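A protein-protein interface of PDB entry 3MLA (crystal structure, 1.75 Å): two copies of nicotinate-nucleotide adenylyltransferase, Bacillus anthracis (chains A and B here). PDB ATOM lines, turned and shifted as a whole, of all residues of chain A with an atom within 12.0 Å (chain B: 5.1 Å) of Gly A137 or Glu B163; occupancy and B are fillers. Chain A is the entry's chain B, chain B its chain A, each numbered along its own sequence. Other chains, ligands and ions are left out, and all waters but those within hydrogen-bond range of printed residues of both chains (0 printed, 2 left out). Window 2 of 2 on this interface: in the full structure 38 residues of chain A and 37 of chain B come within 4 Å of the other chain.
NH1 of Arg B162 is in hydrogen-bond range of OG of Ser B159.
O of Ser B159 is in hydrogen-bond range of N of Lys A139.
The guanidinium group (NH1) of Arg B162 is in hydrogen-bond range of the backbone carbonyl oxygen (O) of Lys A139.
Gly A137 touches Leu B160.
Glu B163 touches Gly A137 (CB to O, 3.4 Å).
CA of Tyr A138 touches O of Ser B159, 3.9 Å away.
Tyr A138 touches Leu B160 (CE1 to CB, 3.8 Å).
CD of Lys A139 touches OE1 of Glu B163 (3.4 Å).
Arg B162 touches Leu A140.
CD of Arg A141 touches CD of Arg B162, at 3.4 Å.
Of the printed residues of chain B, Gly A137 touches Leu B160 (3.8 Å) and Glu B163 (3.4 Å).
Of the printed residues of chain A, Glu B163 touches Gly A137 (3.4 Å) and Lys A139 (3.4 Å).
Ser B159 touches just these residues of chain A: Tyr A138 (3.9 Å) and Lys A139 (3.1 Å).
Of chain A, only Lys A139 (2.8 Å), Leu A140 (3.97 Å) and Arg A141 (3.4 Å) come within 4 Å of Arg B162.
No residue of chain A comes within 4 Å of Glu B167.
Printed residues of chain B within 4 Å of Lys A139: Ser B159, Arg B162 and Glu B163.
Printed residues of chain B within 4 Å of Tyr A138: Ser B159 (3.9 Å) and Leu B160 (3.8 Å).
The nearest residue of chain B that does not touch Gly A137 is Ser B159 (4.2 Å).
The nearest residue of chain A that does not touch Glu B163 is Tyr A138 (4.4 Å).
The nearest printed residue of chain B that does not touch Lys A139 is Leu B160 (4.7 Å).
No position is printed for both chains.
Of the 9 pairs that touch across the chains among the printed residues, none has its exchanged pair printed and touching as well.
Hydrophobic or aromatic side chains of chain A that line the printed part of chain B: Tyr A138.
Among the printed residues, no Asp or Glu carboxylate lies within 4 Å of a Lys or Arg side-chain nitrogen of the other chain.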
ATOM      1  N   GLY A 109      -0.462  25.868  28.248  1.00  0.00           N
ATOM      2  CA  GLY A 109      -0.016  25.662  26.874  1.00  0.00           C
ATOM      3  C   GLY A 109      -1.065  24.989  26.009  1.00  0.00           C
ATOM      4  O   GLY A 109      -1.164  25.274  24.811  1.00  0.00           O
ATOM      5  N   ASP A 110      -1.858  24.103  26.614  1.00  0.00           N
ATOM      6  CA  ASP A 110      -2.973  23.436  25.924  1.00  0.00           C
ATOM      7  C   ASP A 110      -4.117  24.370  25.517  1.00  0.00           C
ATOM      8  O   ASP A 110      -4.889  24.064  24.608  1.00  0.00           O
ATOM      9  CB  ASP A 110      -3.549  22.326  26.809  1.00  0.00           C
ATOM     10  CG  ASP A 110      -2.627  21.127  26.923  1.00  0.00           C
ATOM     11  OD1 ASP A 110      -1.625  21.070  26.177  1.00  0.00           O
ATOM     12  OD2 ASP A 110      -2.910  20.237  27.757  1.00  0.00           O
ATOM     13  N   GLY A 132       1.589  32.184  28.065  1.00  0.00           N
ATOM     14  CA  GLY A 132       1.359  30.760  27.919  1.00  0.00           C
ATOM     15  C   GLY A 132       2.414  29.988  28.687  1.00  0.00           C
ATOM     16  O   GLY A 132       3.607  30.237  28.536  1.00  0.00           O
ATOM     17  N   VAL A 133       1.985  29.053  29.518  1.00  0.00           N
ATOM     18  CA  VAL A 133       2.954  28.235  30.237  1.00  0.00           C
ATOM     19  C   VAL A 133       3.163  26.905  29.511  1.00  0.00           C
ATOM     20  O   VAL A 133       2.211  26.246  29.090  1.00  0.00           O
ATOM     21  CB  VAL A 133       2.618  28.104  31.750  1.00  0.00           C
ATOM     22  CG1 VAL A 133       2.723  29.476  32.417  1.00  0.00           C
ATOM     23  CG2 VAL A 133       1.229  27.531  31.958  1.00  0.00           C
ATOM     24  N   ALA A 134       4.430  26.548  29.324  1.00  0.00           N
ATOM     25  CA  ALA A 134       4.794  25.396  28.508  1.00  0.00           C
ATOM     26  C   ALA A 134       5.831  24.545  29.218  1.00  0.00           C
ATOM     27  O   ALA A 134       6.692  25.064  29.931  1.00  0.00           O
ATOM     28  CB  ALA A 134       5.332  25.850  27.172  1.00  0.00           C
ATOM     29  N   ARG A 135       5.740  23.234  29.017  1.00  0.00           N
ATOM     30  CA  ARG A 135       6.711  22.306  29.583  1.00  0.00           C
ATOM     31  C   ARG A 135       8.059  22.482  28.893  1.00  0.00           C
ATOM     32  O   ARG A 135       8.121  22.868  27.732  1.00  0.00           O
ATOM     33  CB  ARG A 135       6.210  20.864  29.439  1.00  0.00           C
ATOM     34  CG  ARG A 135       4.908  20.594  30.183  1.00  0.00           C
ATOM     35  CD  ARG A 135       4.441  19.150  30.032  1.00  0.00           C
ATOM     36  NE  ARG A 135       3.612  18.946  28.846  1.00  0.00           N
ATOM     37  CZ  ARG A 135       3.006  17.800  28.548  1.00  0.00           C
ATOM     38  NH1 ARG A 135       3.137  16.751  29.352  1.00  0.00           N
ATOM     39  NH2 ARG A 135       2.269  17.699  27.447  1.00  0.00           N
ATOM     40  N   PRO A 136       9.159  22.226  29.620  1.00  0.00           N
ATOM     41  CA  PRO A 136      10.457  22.244  28.940  1.00  0.00           C
ATOM     42  C   PRO A 136      10.389  21.336  27.716  1.00  0.00           C
ATOM     43  O   PRO A 136       9.971  20.186  27.838  1.00  0.00           O
ATOM     44  CB  PRO A 136      11.408  21.654  29.984  1.00  0.00           C
ATOM     45  CG  PRO A 136      10.741  21.921  31.303  1.00  0.00           C
ATOM     46  CD  PRO A 136       9.263  21.835  31.035  1.00  0.00           C
ATOM     47  N   GLY A 137      10.765  21.852  26.551  1.00  0.00           N
ATOM     48  CA  GLY A 137      10.742  21.059  25.334  1.00  0.00           C
ATOM     49  C   GLY A 137       9.486  21.216  24.493  1.00  0.00           C
ATOM     50  O   GLY A 137       9.351  20.588  23.441  1.00  0.00           O
ATOM     51  N   TYR A 138       8.566  22.057  24.950  1.00  0.00           N
ATOM     52  CA  TYR A 138       7.327  22.298  24.219  1.00  0.00           C
ATOM     53  C   TYR A 138       7.303  23.721  23.668  1.00  0.00           C
ATOM     54  O   TYR A 138       7.647  24.675  24.369  1.00  0.00           O
ATOM     55  CB  TYR A 138       6.113  22.031  25.115  1.00  0.00           C
ATOM     56  CG  TYR A 138       5.980  20.580  25.530  1.00  0.00           C
ATOM     57  CD1 TYR A 138       4.836  19.849  25.228  1.00  0.00           C
ATOM     58  CD2 TYR A 138       7.002  19.936  26.213  1.00  0.00           C
ATOM     59  CE1 TYR A 138       4.715  18.520  25.605  1.00  0.00           C
ATOM     60  CE2 TYR A 138       6.892  18.611  26.589  1.00  0.00           C
ATOM     61  CZ  TYR A 138       5.748  17.908  26.283  1.00  0.00           C
ATOM     62  OH  TYR A 138       5.640  16.588  26.659  1.00  0.00           O
ATOM     63  N   LYS A 139       6.908  23.850  22.403  1.00  0.00           N
ATOM     64  CA  LYS A 139       6.896  25.138  21.721  1.00  0.00           C
ATOM     65  C   LYS A 139       5.477  25.564  21.379  1.00  0.00           C
ATOM     66  O   LYS A 139       4.809  24.892  20.602  1.00  0.00           O
ATOM     67  CB  LYS A 139       7.667  25.039  20.408  1.00  0.00           C
ATOM     68  CG  LYS A 139       7.988  26.388  19.787  1.00  0.00           C
ATOM     69  CD  LYS A 139       9.142  27.049  20.539  1.00  0.00           C
ATOM     70  CE  LYS A 139       9.765  28.198  19.754  1.00  0.00           C
ATOM     71  NZ  LYS A 139      11.011  28.687  20.426  1.00  0.00           N
ATOM     72  N   LEU A 140       5.042  26.698  21.918  1.00  0.00           N
ATOM     73  CA  LEU A 140       3.678  27.187  21.680  1.00  0.00           C
ATOM     74  C   LEU A 140       3.547  27.851  20.314  1.00  0.00           C
ATOM     75  O   LEU A 140       4.476  28.505  19.835  1.00  0.00           O
ATOM     76  CB  LEU A 140       3.257  28.163  22.782  1.00  0.00           C
ATOM     77  CG  LEU A 140       3.349  27.625  24.213  1.00  0.00           C
ATOM     78  CD1 LEU A 140       2.898  28.685  25.206  1.00  0.00           C
ATOM     79  CD2 LEU A 140       2.538  26.347  24.378  1.00  0.00           C
ATOM     80  N   ARG A 141       2.385  27.693  19.689  1.00  0.00           N
ATOM     81  CA  ARG A 141       2.185  28.232  18.353  1.00  0.00           C
ATOM     82  C   ARG A 141       0.814  28.892  18.261  1.00  0.00           C
ATOM     83  O   ARG A 141      -0.215  28.254  18.474  1.00  0.00           O
ATOM     84  CB  ARG A 141       2.310  27.114  17.318  1.00  0.00           C
ATOM     85  CG  ARG A 141       2.298  27.578  15.866  1.00  0.00           C
ATOM     86  CD  ARG A 141       2.677  26.413  14.988  1.00  0.00           C
ATOM     87  NE  ARG A 141       2.604  26.692  13.560  1.00  0.00           N
ATOM     88  CZ  ARG A 141       3.662  26.878  12.782  1.00  0.00           C
ATOM     89  NH1 ARG A 141       4.891  26.832  13.299  1.00  0.00           N
ATOM     90  NH2 ARG A 141       3.492  27.110  11.493  1.00  0.00           N
ATOM     91  N   THR A 142       0.806  30.187  17.962  1.00  0.00           N
ATOM     92  CA  THR A 142      -0.434  30.938  17.845  1.00  0.00           C
ATOM     93  C   THR A 142      -0.157  32.155  16.974  1.00  0.00           C
ATOM     94  O   THR A 142       0.953  32.678  16.992  1.00  0.00           O
ATOM     95  CB  THR A 142      -0.929  31.411  19.226  1.00  0.00           C
ATOM     96  OG1 THR A 142      -1.966  32.387  19.069  1.00  0.00           O
ATOM     97  CG2 THR A 142       0.222  32.030  20.017  1.00  0.00           C
ATOM     98  N   THR A 148       5.881  33.391  26.447  1.00  0.00           N
ATOM     99  CA  THR A 148       5.957  32.008  26.911  1.00  0.00           C
ATOM    100  C   THR A 148       6.807  31.927  28.168  1.00  0.00           C
ATOM    101  O   THR A 148       7.878  32.540  28.246  1.00  0.00           O
ATOM    102  CB  THR A 148       6.559  31.079  25.834  1.00  0.00           C
ATOM    103  OG1 THR A 148       5.718  31.083  24.672  1.00  0.00           O
ATOM    104  CG2 THR A 148       6.674  29.650  26.359  1.00  0.00           C
ATOM    105  N   VAL A 149       6.327  31.175  29.149  1.00  0.00           N
ATOM    106  CA  VAL A 149       7.118  30.885  30.338  1.00  0.00           C
ATOM    107  C   VAL A 149       7.247  29.379  30.493  1.00  0.00           C
ATOM    108  O   VAL A 149       6.248  28.654  30.490  1.00  0.00           O
ATOM    109  CB  VAL A 149       6.476  31.475  31.610  1.00  0.00           C
ATOM    110  CG1 VAL A 149       7.244  31.039  32.852  1.00  0.00           C
ATOM    111  CG2 VAL A 149       6.419  32.999  31.519  1.00  0.00           C
ATOM    112  N   GLU A 150       8.480  28.905  30.628  1.00  0.00           N
ATOM    113  CA  GLU A 150       8.703  27.479  30.810  1.00  0.00           C
ATOM    114  C   GLU A 150       8.440  27.066  32.247  1.00  0.00           C
ATOM    115  O   GLU A 150       9.005  27.630  33.181  1.00  0.00           O
ATOM    116  CB  GLU A 150      10.117  27.080  30.366  1.00  0.00           C
ATOM    117  CG  GLU A 150      10.280  27.104  28.842  1.00  0.00           C
ATOM    118  CD  GLU A 150      11.598  26.501  28.381  1.00  0.00           C
ATOM    119  OE1 GLU A 150      12.576  26.550  29.154  1.00  0.00           O
ATOM    120  OE2 GLU A 150      11.655  25.979  27.246  1.00  0.00           O
ATOM    121  N   ILE A 151       7.559  26.090  32.410  1.00  0.00           N
ATOM    122  CA  ILE A 151       7.255  25.533  33.719  1.00  0.00           C
ATOM    123  C   ILE A 151       7.205  24.023  33.599  1.00  0.00           C
ATOM    124  O   ILE A 151       6.457  23.480  32.776  1.00  0.00           O
ATOM    125  CB  ILE A 151       5.871  25.994  34.233  1.00  0.00           C
ATOM    126  CG1 ILE A 151       5.708  27.512  34.074  1.00  0.00           C
ATOM    127  CG2 ILE A 151       5.677  25.585  35.692  1.00  0.00           C
ATOM    128  CD1 ILE A 151       4.566  28.081  34.893  1.00  0.00           C
ATOM    129  N   PRO A 152       7.966  23.333  34.453  1.00  0.00           N
ATOM    130  CA  PRO A 152       7.920  21.869  34.458  1.00  0.00           C
ATOM    131  C   PRO A 152       6.503  21.420  34.759  1.00  0.00           C
ATOM    132  O   PRO A 152       5.864  22.027  35.616  1.00  0.00           O
ATOM    133  CB  PRO A 152       8.809  21.484  35.648  1.00  0.00           C
ATOM    134  CG  PRO A 152       9.440  22.747  36.131  1.00  0.00           C
ATOM    135  CD  PRO A 152       8.599  23.880  35.662  1.00  0.00           C
ATOM    136  N   GLU A 153       6.019  20.389  34.075  1.00  0.00           N
ATOM    137  CA  GLU A 153       4.761  19.767  34.462  1.00  0.00           C
ATOM    138  C   GLU A 153       4.948  19.193  35.867  1.00  0.00           C
ATOM    139  O   GLU A 153       6.049  18.763  36.226  1.00  0.00           O
ATOM    140  CB  GLU A 153       4.378  18.667  33.468  1.00  0.00           C
ATOM    141  CG  GLU A 153       2.956  18.137  33.621  1.00  0.00           C
ATOM    142  CD  GLU A 153       1.901  19.142  33.191  1.00  0.00           C
ATOM    143  OE1 GLU A 153       2.254  20.129  32.508  1.00  0.00           O
ATOM    144  OE2 GLU A 153       0.715  18.942  33.533  1.00  0.00           O
ATOM    145  N   SER B 158       1.383  18.287  20.091  1.00  0.00           N
ATOM    146  CA  SER B 158       1.829  18.985  18.896  1.00  0.00           C
ATOM    147  C   SER B 158       2.970  19.944  19.213  1.00  0.00           C
ATOM    148  O   SER B 158       3.890  20.089  18.415  1.00  0.00           O
ATOM    149  CB  SER B 158       0.660  19.730  18.253  1.00  0.00           C
ATOM    150  OG  SER B 158      -0.326  18.807  17.809  1.00  0.00           O
ATOM    151  N   SER B 159       2.906  20.604  20.367  1.00  0.00           N
ATOM    152  CA  SER B 159       3.966  21.530  20.788  1.00  0.00           C
ATOM    153  C   SER B 159       5.300  20.807  20.939  1.00  0.00           C
ATOM    154  O   SER B 159       6.357  21.341  20.590  1.00  0.00           O
ATOM    155  CB  SER B 159       3.595  22.188  22.114  1.00  0.00           C
ATOM    156  OG  SER B 159       2.359  22.877  22.018  1.00  0.00           O
ATOM    157  N   LEU B 160       5.243  19.591  21.465  1.00  0.00           N
ATOM    158  CA  LEU B 160       6.431  18.752  21.578  1.00  0.00           C
ATOM    159  C   LEU B 160       6.989  18.464  20.195  1.00  0.00           C
ATOM    160  O   LEU B 160       8.169  18.670  19.944  1.00  0.00           O
ATOM    161  CB  LEU B 160       6.096  17.431  22.272  1.00  0.00           C
ATOM    162  CG  LEU B 160       7.228  16.394  22.222  1.00  0.00           C
ATOM    163  CD1 LEU B 160       8.470  16.942  22.907  1.00  0.00           C
ATOM    164  CD2 LEU B 160       6.804  15.076  22.846  1.00  0.00           C
ATOM    165  N   LEU B 161       6.125  18.003  19.291  1.00  0.00           N
ATOM    166  CA  LEU B 161       6.565  17.591  17.955  1.00  0.00           C
ATOM    167  C   LEU B 161       7.123  18.740  17.121  1.00  0.00           C
ATOM    168  O   LEU B 161       8.100  18.575  16.374  1.00  0.00           O
ATOM    169  CB  LEU B 161       5.415  16.926  17.189  1.00  0.00           C
ATOM    170  CG  LEU B 161       4.737  15.727  17.860  1.00  0.00           C
ATOM    171  CD1 LEU B 161       3.742  15.090  16.911  1.00  0.00           C
ATOM    172  CD2 LEU B 161       5.756  14.722  18.307  1.00  0.00           C
ATOM    173  N   ARG B 162       6.492  19.902  17.224  1.00  0.00           N
ATOM    174  CA  ARG B 162       6.970  21.041  16.462  1.00  0.00           C
ATOM    175  C   ARG B 162       8.398  21.409  16.871  1.00  0.00           C
ATOM    176  O   ARG B 162       9.233  21.682  16.017  1.00  0.00           O
ATOM    177  CB  ARG B 162       6.036  22.231  16.621  1.00  0.00           C
ATOM    178  CG  ARG B 162       4.693  22.049  15.926  1.00  0.00           C
ATOM    179  CD  ARG B 162       3.903  23.355  15.958  1.00  0.00           C
ATOM    180  NE  ARG B 162       3.705  23.818  17.331  1.00  0.00           N
ATOM    181  CZ  ARG B 162       2.566  23.725  18.002  1.00  0.00           C
ATOM    182  NH1 ARG B 162       2.498  24.178  19.242  1.00  0.00           N
ATOM    183  NH2 ARG B 162       1.481  23.195  17.436  1.00  0.00           N
ATOM    184  N   GLU B 163       8.661  21.411  18.176  1.00  0.00           N
ATOM    185  CA  GLU B 163      10.005  21.687  18.693  1.00  0.00           C
ATOM    186  C   GLU B 163      11.018  20.692  18.134  1.00  0.00           C
ATOM    187  O   GLU B 163      12.114  21.066  17.715  1.00  0.00           O
ATOM    188  CB  GLU B 163      10.016  21.629  20.221  1.00  0.00           C
ATOM    189  CG  GLU B 163      11.369  21.962  20.843  1.00  0.00           C
ATOM    190  CD  GLU B 163      11.705  23.443  20.761  1.00  0.00           C
ATOM    191  OE1 GLU B 163      10.932  24.259  21.309  1.00  0.00           O
ATOM    192  OE2 GLU B 163      12.746  23.793  20.159  1.00  0.00           O
ATOM    193  N   ARG B 164      10.659  19.411  18.141  1.00  0.00           N
ATOM    194  CA  ARG B 164      11.536  18.401  17.554  1.00  0.00           C
ATOM    195  C   ARG B 164      11.824  18.697  16.079  1.00  0.00           C
ATOM    196  O   ARG B 164      12.976  18.640  15.652  1.00  0.00           O
ATOM    197  CB  ARG B 164      10.967  16.981  17.731  1.00  0.00           C
ATOM    198  CG  ARG B 164      10.889  16.519  19.181  1.00  0.00           C
ATOM    199  CD  ARG B 164      10.334  15.097  19.295  1.00  0.00           C
ATOM    200  NE  ARG B 164      11.164  14.130  18.582  1.00  0.00           N
ATOM    201  CZ  ARG B 164      12.252  13.560  19.093  1.00  0.00           C
ATOM    202  NH1 ARG B 164      12.643  13.859  20.327  1.00  0.00           N
ATOM    203  NH2 ARG B 164      12.959  12.701  18.372  1.00  0.00           N
ATOM    204  N   TYR B 165      10.791  19.037  15.303  1.00  0.00           N
ATOM    205  CA  TYR B 165      10.996  19.323  13.878  1.00  0.00           C
ATOM    206  C   TYR B 165      11.864  20.565  13.681  1.00  0.00           C
ATOM    207  O   TYR B 165      12.668  20.638  12.743  1.00  0.00           O
ATOM    208  CB  TYR B 165       9.662  19.472  13.125  1.00  0.00           C
ATOM    209  CG  TYR B 165       8.964  18.151  12.862  1.00  0.00           C
ATOM    210  CD1 TYR B 165       7.729  17.868  13.437  1.00  0.00           C
ATOM    211  CD2 TYR B 165       9.546  17.185  12.049  1.00  0.00           C
ATOM    212  CE1 TYR B 165       7.096  16.661  13.212  1.00  0.00           C
ATOM    213  CE2 TYR B 165       8.924  15.973  11.815  1.00  0.00           C
ATOM    214  CZ  TYR B 165       7.696  15.719  12.403  1.00  0.00           C
ATOM    215  OH  TYR B 165       7.068  14.519  12.179  1.00  0.00           O
ATOM    216  N   LYS B 166      11.703  21.532  14.581  1.00  0.00           N
ATOM    217  CA  LYS B 166      12.507  22.750  14.563  1.00  0.00           C
ATOM    218  C   LYS B 166      13.970  22.374  14.771  1.00  0.00           C
ATOM    219  O   LYS B 166      14.873  23.018  14.237  1.00  0.00           O
ATOM    220  CB  LYS B 166      12.046  23.704  15.670  1.00  0.00           C
ATOM    221  CG  LYS B 166      12.329  25.187  15.407  1.00  0.00           C
ATOM    222  CD  LYS B 166      13.770  25.559  15.690  1.00  0.00           C
ATOM    223  CE  LYS B 166      13.988  27.058  15.533  1.00  0.00           C
ATOM    224  NZ  LYS B 166      15.355  27.475  15.961  1.00  0.00           N
ATOM    225  N   GLU B 167      14.194  21.330  15.557  1.00  0.00           N
ATOM    226  CA  GLU B 167      15.541  20.841  15.820  1.00  0.00           C
ATOM    227  C   GLU B 167      15.962  19.795  14.792  1.00  0.00           C
ATOM    228  O   GLU B 167      17.008  19.167  14.929  1.00  0.00           O
ATOM    229  CB  GLU B 167      15.637  20.257  17.231  1.00  0.00           C
ATOM    230  CG  GLU B 167      15.385  21.247  18.353  1.00  0.00           C
ATOM    231  CD  GLU B 167      15.672  20.651  19.716  1.00  0.00           C
ATOM    232  OE1 GLU B 167      16.681  19.926  19.843  1.00  0.00           O
ATOM    233  OE2 GLU B 167      14.894  20.903  20.661  1.00  0.00           O
